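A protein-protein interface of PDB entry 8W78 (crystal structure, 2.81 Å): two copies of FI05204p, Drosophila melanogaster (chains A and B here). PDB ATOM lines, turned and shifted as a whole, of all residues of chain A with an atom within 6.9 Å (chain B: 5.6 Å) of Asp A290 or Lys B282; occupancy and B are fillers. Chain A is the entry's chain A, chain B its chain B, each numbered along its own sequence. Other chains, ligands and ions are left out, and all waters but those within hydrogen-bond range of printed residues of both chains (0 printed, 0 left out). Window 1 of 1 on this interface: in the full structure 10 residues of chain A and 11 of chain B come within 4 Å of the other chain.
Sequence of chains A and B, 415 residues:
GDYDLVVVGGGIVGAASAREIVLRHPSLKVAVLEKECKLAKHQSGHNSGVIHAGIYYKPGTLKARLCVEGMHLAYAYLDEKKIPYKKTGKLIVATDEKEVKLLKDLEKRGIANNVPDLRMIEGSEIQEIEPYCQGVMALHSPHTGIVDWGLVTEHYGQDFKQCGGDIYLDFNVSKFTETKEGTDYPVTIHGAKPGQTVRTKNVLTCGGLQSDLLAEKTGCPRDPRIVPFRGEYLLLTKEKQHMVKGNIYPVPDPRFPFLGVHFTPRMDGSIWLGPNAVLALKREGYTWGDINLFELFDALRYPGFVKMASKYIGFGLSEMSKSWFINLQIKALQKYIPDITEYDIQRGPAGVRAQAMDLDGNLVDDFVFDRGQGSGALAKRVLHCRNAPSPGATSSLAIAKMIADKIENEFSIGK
Among the printed residues, pairs that only touch across the chains: Gly A289 with Ile B291, Gly A289 with Asn B292, Ile A291 with Asp B290, Ile A291 with Leu B293 and Asn A292 with Asp B290.
Of the 13 printed residues of chain B, 5 touch a printed residue of chain A.
Hydrophobic or aromatic side chains of chain B that line the printed part of chain A: Ile B291 and Leu B293.
Along chain B the printed residues that touch a printed residue of chain A span positions 282 to 293.
Of the 13 printed residues of chain A, 5 touch a printed residue of chain B.
Hydrophobic or aromatic side chains of chain A within 4 Å of the printed part of chain B: Ile A291.
The side-chain amino group (NZ) of Lys A282 lies within salt-bridge range of the side-chain carboxylate (OD1) of Asp B290 (3.2 Å).
The backbone carbonyl oxygen (O) of Gly A289 lies within hydrogen-bond range of the backbone NH (N) of Leu B293, at 3.0 Å.
The side-chain carboxylate (OD2) of Asp A290 is in salt-bridge range of the side-chain amino group (NZ) of Lys B282 (3.2 Å).
The side-chain amide nitrogen (ND2) of Asn B292 sits close to the backbone NH (N) of Asp A290 (3.5 Å).
O of Ile B291 sits at hydrogen-bond distance from N of Ile A291, at 2.9 Å.
The side-chain carboxylate (OD1) of Asp A290 lies close to the backbone carbonyl oxygen (O) of Ile B291 (3.3 Å).
Of chain B, only Lys B282 (3.2 Å), Ile B291 (3.3 Å) and Asn B292 (3.5 Å) come within 4 Å of Asp A290.
Of chain A, only Asp A290 (3.2 Å) comes within 4 Å of Lys B282.
Of the printed residues of chain B, Asn A292 touches Asp B290 (3.6 Å).
Printed residues of chain B within 4 Å of Gly A289: Ile B291, Asn B292 and Leu B293.
Of the printed residues of chain B, Ile A291 touches Asp B290 (3.8 Å), Ile B291 (2.9 Å) and Leu B293 (3.8 Å).
Of the printed residues of chain A, Asp B290 touches Lys A282 (3.2 Å), Ile A291 (3.8 Å) and Asn A292 (3.6 Å).
Printed residues of chain A within 4 Å of Asn B292: Gly A289 and Asp A290.
Pro B228 touches none of the printed residues of chain A.
Thr A287 touches none of the printed residues of chain B.
The nearest residue of chain B that does not touch Asp A290 is Asp B290 (4.6 Å).
The nearest residue of chain A that does not touch Lys B282 is Lys A282 (4.2 Å).
The nearest printed residue of chain A that does not touch Asp B290 is Asp A290 (4.6 Å).
Lys A282 touches Asp B290, and with the chains exchanged Asp A290 touches Lys B282.
Asp A290 touches Ile B291, and with the chains exchanged Ile A291 touches Asp B290.
Asp A290 touches Asn B292, and with the chains exchanged Asn A292 touches Asp B290.
Ile B291 touches its own counterpart, Ile A291.
8 positions are printed for both chains.
N of Asn A292 lies within hydrogen-bond range of O of Leu A281 (3.0 Å).
N of Asn B292 is in hydrogen-bond range of O of Leu B281 (3.1 Å).
The side-chain amide oxygen (OD1) of Asn B292 is in hydrogen-bond range of the backbone NH (N) of Glu B295 (2.6 Å).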
ATOM      1  N   ARG A 230      -2.911 -10.003  14.877  1.00  0.00           N
ATOM      2  CA  ARG A 230      -2.582 -10.852  16.013  1.00  0.00           C
ATOM      3  C   ARG A 230      -3.507 -10.565  17.190  1.00  0.00           C
ATOM      4  O   ARG A 230      -3.802  -9.409  17.505  1.00  0.00           O
ATOM      5  CB  ARG A 230      -1.125 -10.650  16.430  1.00  0.00           C
ATOM      6  CG  ARG A 230      -0.713 -11.484  17.636  1.00  0.00           C
ATOM      7  CD  ARG A 230       0.771 -11.360  17.946  1.00  0.00           C
ATOM      8  NE  ARG A 230       1.157  -9.997  18.301  1.00  0.00           N
ATOM      9  CZ  ARG A 230       1.810  -9.171  17.491  1.00  0.00           C
ATOM     10  NH1 ARG A 230       2.156  -9.567  16.274  1.00  0.00           N
ATOM     11  NH2 ARG A 230       2.119  -7.949  17.900  1.00  0.00           N
ATOM     12  N   ALA A 280      -0.255  -7.610  12.922  1.00  0.00           N
ATOM     13  CA  ALA A 280       0.958  -8.413  12.966  1.00  0.00           C
ATOM     14  C   ALA A 280       1.859  -8.081  11.785  1.00  0.00           C
ATOM     15  O   ALA A 280       1.397  -7.951  10.648  1.00  0.00           O
ATOM     16  CB  ALA A 280       0.615  -9.903  12.962  1.00  0.00           C
ATOM     17  N   LEU A 281       3.157  -7.938  12.064  1.00  0.00           N
ATOM     18  CA  LEU A 281       4.154  -7.664  11.035  1.00  0.00           C
ATOM     19  C   LEU A 281       4.666  -8.935  10.367  1.00  0.00           C
ATOM     20  O   LEU A 281       5.834  -8.992   9.960  1.00  0.00           O
ATOM     21  CB  LEU A 281       5.314  -6.868  11.634  1.00  0.00           C
ATOM     22  CG  LEU A 281       4.925  -5.558  12.325  1.00  0.00           C
ATOM     23  CD1 LEU A 281       6.152  -4.841  12.863  1.00  0.00           C
ATOM     24  CD2 LEU A 281       4.148  -4.658  11.377  1.00  0.00           C
ATOM     25  N   LYS A 282       3.814  -9.950  10.243  1.00  0.00           N
ATOM     26  CA  LYS A 282       4.163 -11.251   9.689  1.00  0.00           C
ATOM     27  C   LYS A 282       2.887 -12.073   9.587  1.00  0.00           C
ATOM     28  O   LYS A 282       1.992 -11.946  10.429  1.00  0.00           O
ATOM     29  CB  LYS A 282       5.196 -11.973  10.565  1.00  0.00           C
ATOM     30  CG  LYS A 282       5.755 -13.254   9.973  1.00  0.00           C
ATOM     31  CD  LYS A 282       6.545 -14.028  11.016  1.00  0.00           C
ATOM     32  CE  LYS A 282       7.901 -14.458  10.484  1.00  0.00           C
ATOM     33  NZ  LYS A 282       7.791 -15.368   9.312  1.00  0.00           N
ATOM     34  N   GLU A 284       2.551 -15.301  10.051  1.00  0.00           N
ATOM     35  CA  GLU A 284       2.557 -16.095  11.278  1.00  0.00           C
ATOM     36  C   GLU A 284       3.248 -15.355  12.416  1.00  0.00           C
ATOM     37  O   GLU A 284       3.996 -15.952  13.197  1.00  0.00           O
ATOM     38  CB  GLU A 284       3.218 -17.447  11.035  1.00  0.00           C
ATOM     39  CG  GLU A 284       2.459 -18.350  10.075  1.00  0.00           C
ATOM     40  CD  GLU A 284       3.117 -19.706   9.907  1.00  0.00           C
ATOM     41  OE1 GLU A 284       4.234 -19.896  10.433  1.00  0.00           O
ATOM     42  OE2 GLU A 284       2.517 -20.583   9.252  1.00  0.00           O
ATOM     43  N   GLY A 285       3.017 -14.051  12.527  1.00  0.00           N
ATOM     44  CA  GLY A 285       3.636 -13.260  13.570  1.00  0.00           C
ATOM     45  C   GLY A 285       2.928 -13.376  14.902  1.00  0.00           C
ATOM     46  O   GLY A 285       2.105 -12.525  15.252  1.00  0.00           O
ATOM     47  N   TYR A 286       3.239 -14.431  15.656  1.00  0.00           N
ATOM     48  CA  TYR A 286       2.632 -14.633  16.965  1.00  0.00           C
ATOM     49  C   TYR A 286       3.270 -13.783  18.054  1.00  0.00           C
ATOM     50  O   TYR A 286       2.730 -13.722  19.164  1.00  0.00           O
ATOM     51  CB  TYR A 286       2.704 -16.112  17.355  1.00  0.00           C
ATOM     52  CG  TYR A 286       1.836 -17.007  16.499  1.00  0.00           C
ATOM     53  CD1 TYR A 286       0.518 -17.269  16.851  1.00  0.00           C
ATOM     54  CD2 TYR A 286       2.333 -17.588  15.340  1.00  0.00           C
ATOM     55  CE1 TYR A 286      -0.280 -18.085  16.072  1.00  0.00           C
ATOM     56  CE2 TYR A 286       1.541 -18.405  14.555  1.00  0.00           C
ATOM     57  CZ  TYR A 286       0.237 -18.650  14.926  1.00  0.00           C
ATOM     58  OH  TYR A 286      -0.553 -19.462  14.147  1.00  0.00           O
ATOM     59  N   THR A 287       4.392 -13.129  17.770  1.00  0.00           N
ATOM     60  CA  THR A 287       5.074 -12.269  18.724  1.00  0.00           C
ATOM     61  C   THR A 287       5.213 -10.866  18.147  1.00  0.00           C
ATOM     62  O   THR A 287       5.018 -10.634  16.952  1.00  0.00           O
ATOM     63  CB  THR A 287       6.455 -12.828  19.094  1.00  0.00           C
ATOM     64  OG1 THR A 287       7.230 -13.022  17.904  1.00  0.00           O
ATOM     65  CG2 THR A 287       6.315 -14.153  19.828  1.00  0.00           C
ATOM     66  N   TRP A 288       5.560  -9.922  19.023  1.00  0.00           N
ATOM     67  CA  TRP A 288       5.700  -8.534  18.602  1.00  0.00           C
ATOM     68  C   TRP A 288       6.984  -8.289  17.821  1.00  0.00           C
ATOM     69  O   TRP A 288       7.047  -7.328  17.045  1.00  0.00           O
ATOM     70  CB  TRP A 288       5.660  -7.608  19.816  1.00  0.00           C
ATOM     71  CG  TRP A 288       4.475  -6.688  19.857  1.00  0.00           C
ATOM     72  CD1 TRP A 288       3.560  -6.574  20.864  1.00  0.00           C
ATOM     73  CD2 TRP A 288       4.076  -5.752  18.846  1.00  0.00           C
ATOM     74  NE1 TRP A 288       2.620  -5.625  20.544  1.00  0.00           N
ATOM     75  CE2 TRP A 288       2.914  -5.107  19.310  1.00  0.00           C
ATOM     76  CE3 TRP A 288       4.589  -5.398  17.593  1.00  0.00           C
ATOM     77  CZ2 TRP A 288       2.258  -4.125  18.570  1.00  0.00           C
ATOM     78  CZ3 TRP A 288       3.934  -4.427  16.858  1.00  0.00           C
ATOM     79  CH2 TRP A 288       2.781  -3.803  17.349  1.00  0.00           C
ATOM     80  N   GLY A 289       7.999  -9.127  18.002  1.00  0.00           N
ATOM     81  CA  GLY A 289       9.300  -8.867  17.418  1.00  0.00           C
ATOM     82  C   GLY A 289       9.531  -9.501  16.062  1.00  0.00           C
ATOM     83  O   GLY A 289      10.325  -8.992  15.266  1.00  0.00           O
ATOM     84  N   ASP A 290       8.847 -10.609  15.784  1.00  0.00           N
ATOM     85  CA  ASP A 290       9.063 -11.337  14.539  1.00  0.00           C
ATOM     86  C   ASP A 290       8.458 -10.553  13.381  1.00  0.00           C
ATOM     87  O   ASP A 290       7.237 -10.384  13.303  1.00  0.00           O
ATOM     88  CB  ASP A 290       8.460 -12.735  14.636  1.00  0.00           C
ATOM     89  CG  ASP A 290       9.242 -13.760  13.837  1.00  0.00           C
ATOM     90  OD1 ASP A 290       9.808 -13.392  12.787  1.00  0.00           O
ATOM     91  OD2 ASP A 290       9.300 -14.932  14.265  1.00  0.00           O
ATOM     92  N   ILE A 291       9.311 -10.071  12.480  1.00  0.00           N
ATOM     93  CA  ILE A 291       8.897  -9.258  11.343  1.00  0.00           C
ATOM     94  C   ILE A 291       9.407  -9.910  10.065  1.00  0.00           C
ATOM     95  O   ILE A 291      10.522 -10.444  10.031  1.00  0.00           O
ATOM     96  CB  ILE A 291       9.420  -7.810  11.459  1.00  0.00           C
ATOM     97  CG1 ILE A 291       9.085  -7.221  12.830  1.00  0.00           C
ATOM     98  CG2 ILE A 291       8.838  -6.936  10.358  1.00  0.00           C
ATOM     99  CD1 ILE A 291       9.690  -5.856  13.066  1.00  0.00           C
ATOM    100  N   ASN A 292       8.587  -9.869   9.017  1.00  0.00           N
ATOM    101  CA  ASN A 292       8.972 -10.325   7.685  1.00  0.00           C
ATOM    102  C   ASN A 292       8.901  -9.120   6.754  1.00  0.00           C
ATOM    103  O   ASN A 292       7.812  -8.600   6.487  1.00  0.00           O
ATOM    104  CB  ASN A 292       8.066 -11.457   7.203  1.00  0.00           C
ATOM    105  CG  ASN A 292       8.643 -12.202   6.015  1.00  0.00           C
ATOM    106  OD1 ASN A 292       9.251 -11.605   5.126  1.00  0.00           O
ATOM    107  ND2 ASN A 292       8.456 -13.517   5.995  1.00  0.00           N
ATOM    108  N   PRO B 228      23.977 -15.975  14.268  1.00  0.00           N
ATOM    109  CA  PRO B 228      23.496 -16.678  13.071  1.00  0.00           C
ATOM    110  C   PRO B 228      24.105 -16.098  11.802  1.00  0.00           C
ATOM    111  O   PRO B 228      24.047 -14.889  11.564  1.00  0.00           O
ATOM    112  CB  PRO B 228      21.976 -16.456  13.112  1.00  0.00           C
ATOM    113  CG  PRO B 228      21.717 -15.509  14.288  1.00  0.00           C
ATOM    114  CD  PRO B 228      23.032 -14.939  14.705  1.00  0.00           C
ATOM    115  N   ALA B 280      22.555 -13.085   9.721  1.00  0.00           N
ATOM    116  CA  ALA B 280      21.115 -13.281   9.791  1.00  0.00           C
ATOM    117  C   ALA B 280      20.525 -12.442  10.915  1.00  0.00           C
ATOM    118  O   ALA B 280      20.991 -12.498  12.058  1.00  0.00           O
ATOM    119  CB  ALA B 280      20.787 -14.758  10.002  1.00  0.00           C
ATOM    120  N   LEU B 281      19.496 -11.661  10.590  1.00  0.00           N
ATOM    121  CA  LEU B 281      18.769 -10.879  11.583  1.00  0.00           C
ATOM    122  C   LEU B 281      17.794 -11.727  12.391  1.00  0.00           C
ATOM    123  O   LEU B 281      16.922 -11.175  13.070  1.00  0.00           O
ATOM    124  CB  LEU B 281      18.029  -9.727  10.900  1.00  0.00           C
ATOM    125  CG  LEU B 281      18.914  -8.804  10.056  1.00  0.00           C
ATOM    126  CD1 LEU B 281      18.107  -7.667   9.449  1.00  0.00           C
ATOM    127  CD2 LEU B 281      20.069  -8.263  10.886  1.00  0.00           C
ATOM    128  N   LYS B 282      17.930 -13.049  12.327  1.00  0.00           N
ATOM    129  CA  LYS B 282      17.077 -13.978  13.049  1.00  0.00           C
ATOM    130  C   LYS B 282      17.845 -15.282  13.204  1.00  0.00           C
ATOM    131  O   LYS B 282      18.537 -15.710  12.276  1.00  0.00           O
ATOM    132  CB  LYS B 282      15.754 -14.208  12.310  1.00  0.00           C
ATOM    133  CG  LYS B 282      14.769 -15.114  13.026  1.00  0.00           C
ATOM    134  CD  LYS B 282      13.498 -15.279  12.207  1.00  0.00           C
ATOM    135  CE  LYS B 282      12.483 -16.159  12.918  1.00  0.00           C
ATOM    136  NZ  LYS B 282      11.242 -16.325  12.112  1.00  0.00           N
ATOM    137  N   ARG B 283      17.729 -15.900  14.383  1.00  0.00           N
ATOM    138  CA  ARG B 283      18.490 -17.114  14.665  1.00  0.00           C
ATOM    139  C   ARG B 283      18.178 -18.210  13.654  1.00  0.00           C
ATOM    140  O   ARG B 283      19.088 -18.848  13.110  1.00  0.00           O
ATOM    141  CB  ARG B 283      18.205 -17.588  16.088  1.00  0.00           C
ATOM    142  CG  ARG B 283      18.778 -16.672  17.149  1.00  0.00           C
ATOM    143  CD  ARG B 283      19.917 -17.343  17.885  1.00  0.00           C
ATOM    144  NE  ARG B 283      20.581 -16.426  18.802  1.00  0.00           N
ATOM    145  CZ  ARG B 283      21.212 -16.812  19.904  1.00  0.00           C
ATOM    146  NH1 ARG B 283      21.251 -18.095  20.230  1.00  0.00           N
ATOM    147  NH2 ARG B 283      21.794 -15.916  20.685  1.00  0.00           N
ATOM    148  N   GLU B 284      16.896 -18.444  13.389  1.00  0.00           N
ATOM    149  CA  GLU B 284      16.468 -19.342  12.318  1.00  0.00           C
ATOM    150  C   GLU B 284      16.053 -18.562  11.079  1.00  0.00           C
ATOM    151  O   GLU B 284      15.078 -18.910  10.407  1.00  0.00           O
ATOM    152  CB  GLU B 284      15.336 -20.245  12.797  1.00  0.00           C
ATOM    153  CG  GLU B 284      15.743 -21.218  13.891  1.00  0.00           C
ATOM    154  CD  GLU B 284      14.671 -22.248  14.185  1.00  0.00           C
ATOM    155  OE1 GLU B 284      13.659 -22.280  13.454  1.00  0.00           O
ATOM    156  OE2 GLU B 284      14.840 -23.025  15.148  1.00  0.00           O
ATOM    157  N   GLY B 285      16.780 -17.493  10.765  1.00  0.00           N
ATOM    158  CA  GLY B 285      16.466 -16.666   9.618  1.00  0.00           C
ATOM    159  C   GLY B 285      17.026 -17.210   8.321  1.00  0.00           C
ATOM    160  O   GLY B 285      18.153 -16.885   7.936  1.00  0.00           O
ATOM    161  N   ASP B 290      13.319 -12.153   7.040  1.00  0.00           N
ATOM    162  CA  ASP B 290      12.996 -12.719   8.348  1.00  0.00           C
ATOM    163  C   ASP B 290      13.886 -12.083   9.407  1.00  0.00           C
ATOM    164  O   ASP B 290      15.068 -12.414   9.527  1.00  0.00           O
ATOM    165  CB  ASP B 290      13.163 -14.234   8.330  1.00  0.00           C
ATOM    166  CG  ASP B 290      11.885 -14.956   7.957  1.00  0.00           C
ATOM    167  OD1 ASP B 290      10.820 -14.602   8.507  1.00  0.00           O
ATOM    168  OD2 ASP B 290      11.943 -15.873   7.112  1.00  0.00           O
ATOM    169  N   ILE B 291      13.319 -11.158  10.180  1.00  0.00           N
ATOM    170  CA  ILE B 291      14.026 -10.515  11.277  1.00  0.00           C
ATOM    171  C   ILE B 291      13.216 -10.705  12.553  1.00  0.00           C
ATOM    172  O   ILE B 291      12.016 -10.989  12.525  1.00  0.00           O
ATOM    173  CB  ILE B 291      14.285  -9.016  11.017  1.00  0.00           C
ATOM    174  CG1 ILE B 291      13.057  -8.184  11.392  1.00  0.00           C
ATOM    175  CG2 ILE B 291      14.648  -8.777   9.559  1.00  0.00           C
ATOM    176  CD1 ILE B 291      13.268  -6.693  11.255  1.00  0.00           C
ATOM    177  N   ASN B 292      13.897 -10.550  13.687  1.00  0.00           N
ATOM    178  CA  ASN B 292      13.262 -10.623  14.999  1.00  0.00           C
ATOM    179  C   ASN B 292      13.907  -9.580  15.894  1.00  0.00           C
ATOM    180  O   ASN B 292      15.115  -9.635  16.137  1.00  0.00           O
ATOM    181  CB  ASN B 292      13.399 -12.020  15.612  1.00  0.00           C
ATOM    182  CG  ASN B 292      12.712 -12.132  16.958  1.00  0.00           C
ATOM    183  OD1 ASN B 292      13.288 -11.797  17.992  1.00  0.00           O
ATOM    184  ND2 ASN B 292      11.471 -12.607  16.952  1.00  0.00           N
ATOM    185  N   LEU B 293      13.100  -8.634  16.384  1.00  0.00           N
ATOM    186  CA  LEU B 293      13.645  -7.532  17.170  1.00  0.00           C
ATOM    187  C   LEU B 293      14.231  -8.020  18.489  1.00  0.00           C
ATOM    188  O   LEU B 293      15.247  -7.491  18.955  1.00  0.00           O
ATOM    189  CB  LEU B 293      12.561  -6.482  17.418  1.00  0.00           C
ATOM    190  CG  LEU B 293      11.903  -5.904  16.165  1.00  0.00           C
ATOM    191  CD1 LEU B 293      10.894  -4.828  16.532  1.00  0.00           C
ATOM    192  CD2 LEU B 293      12.955  -5.359  15.211  1.00  0.00           C
ATOM    193  N   GLU B 295      15.508 -11.154  19.137  1.00  0.00           N
ATOM    194  CA  GLU B 295      16.739 -11.873  18.831  1.00  0.00           C
ATOM    195  C   GLU B 295      17.819 -10.973  18.248  1.00  0.00           C
ATOM    196  O   GLU B 295      18.981 -11.390  18.188  1.00  0.00           O
ATOM    197  CB  GLU B 295      16.450 -13.025  17.866  1.00  0.00           C
ATOM    198  CG  GLU B 295      15.547 -14.104  18.442  1.00  0.00           C
ATOM    199  CD  GLU B 295      15.277 -15.226  17.459  1.00  0.00           C
ATOM    200  OE1 GLU B 295      14.519 -16.156  17.811  1.00  0.00           O
ATOM    201  OE2 GLU B 295      15.821 -15.179  16.335  1.00  0.00           O
ATOM    202  N   VAL B 352      21.587 -21.722   7.940  1.00  0.00           N
ATOM    203  CA  VAL B 352      22.056 -20.800   8.968  1.00  0.00           C
ATOM    204  C   VAL B 352      23.109 -21.510   9.807  1.00  0.00           C
ATOM    205  O   VAL B 352      22.907 -22.654  10.232  1.00  0.00           O
ATOM    206  CB  VAL B 352      20.897 -20.297   9.845  1.00  0.00           C
ATOM    207  CG1 VAL B 352      21.373 -19.181  10.760  1.00  0.00           C
ATOM    208  CG2 VAL B 352      19.740 -19.828   8.978  1.00  0.00           C
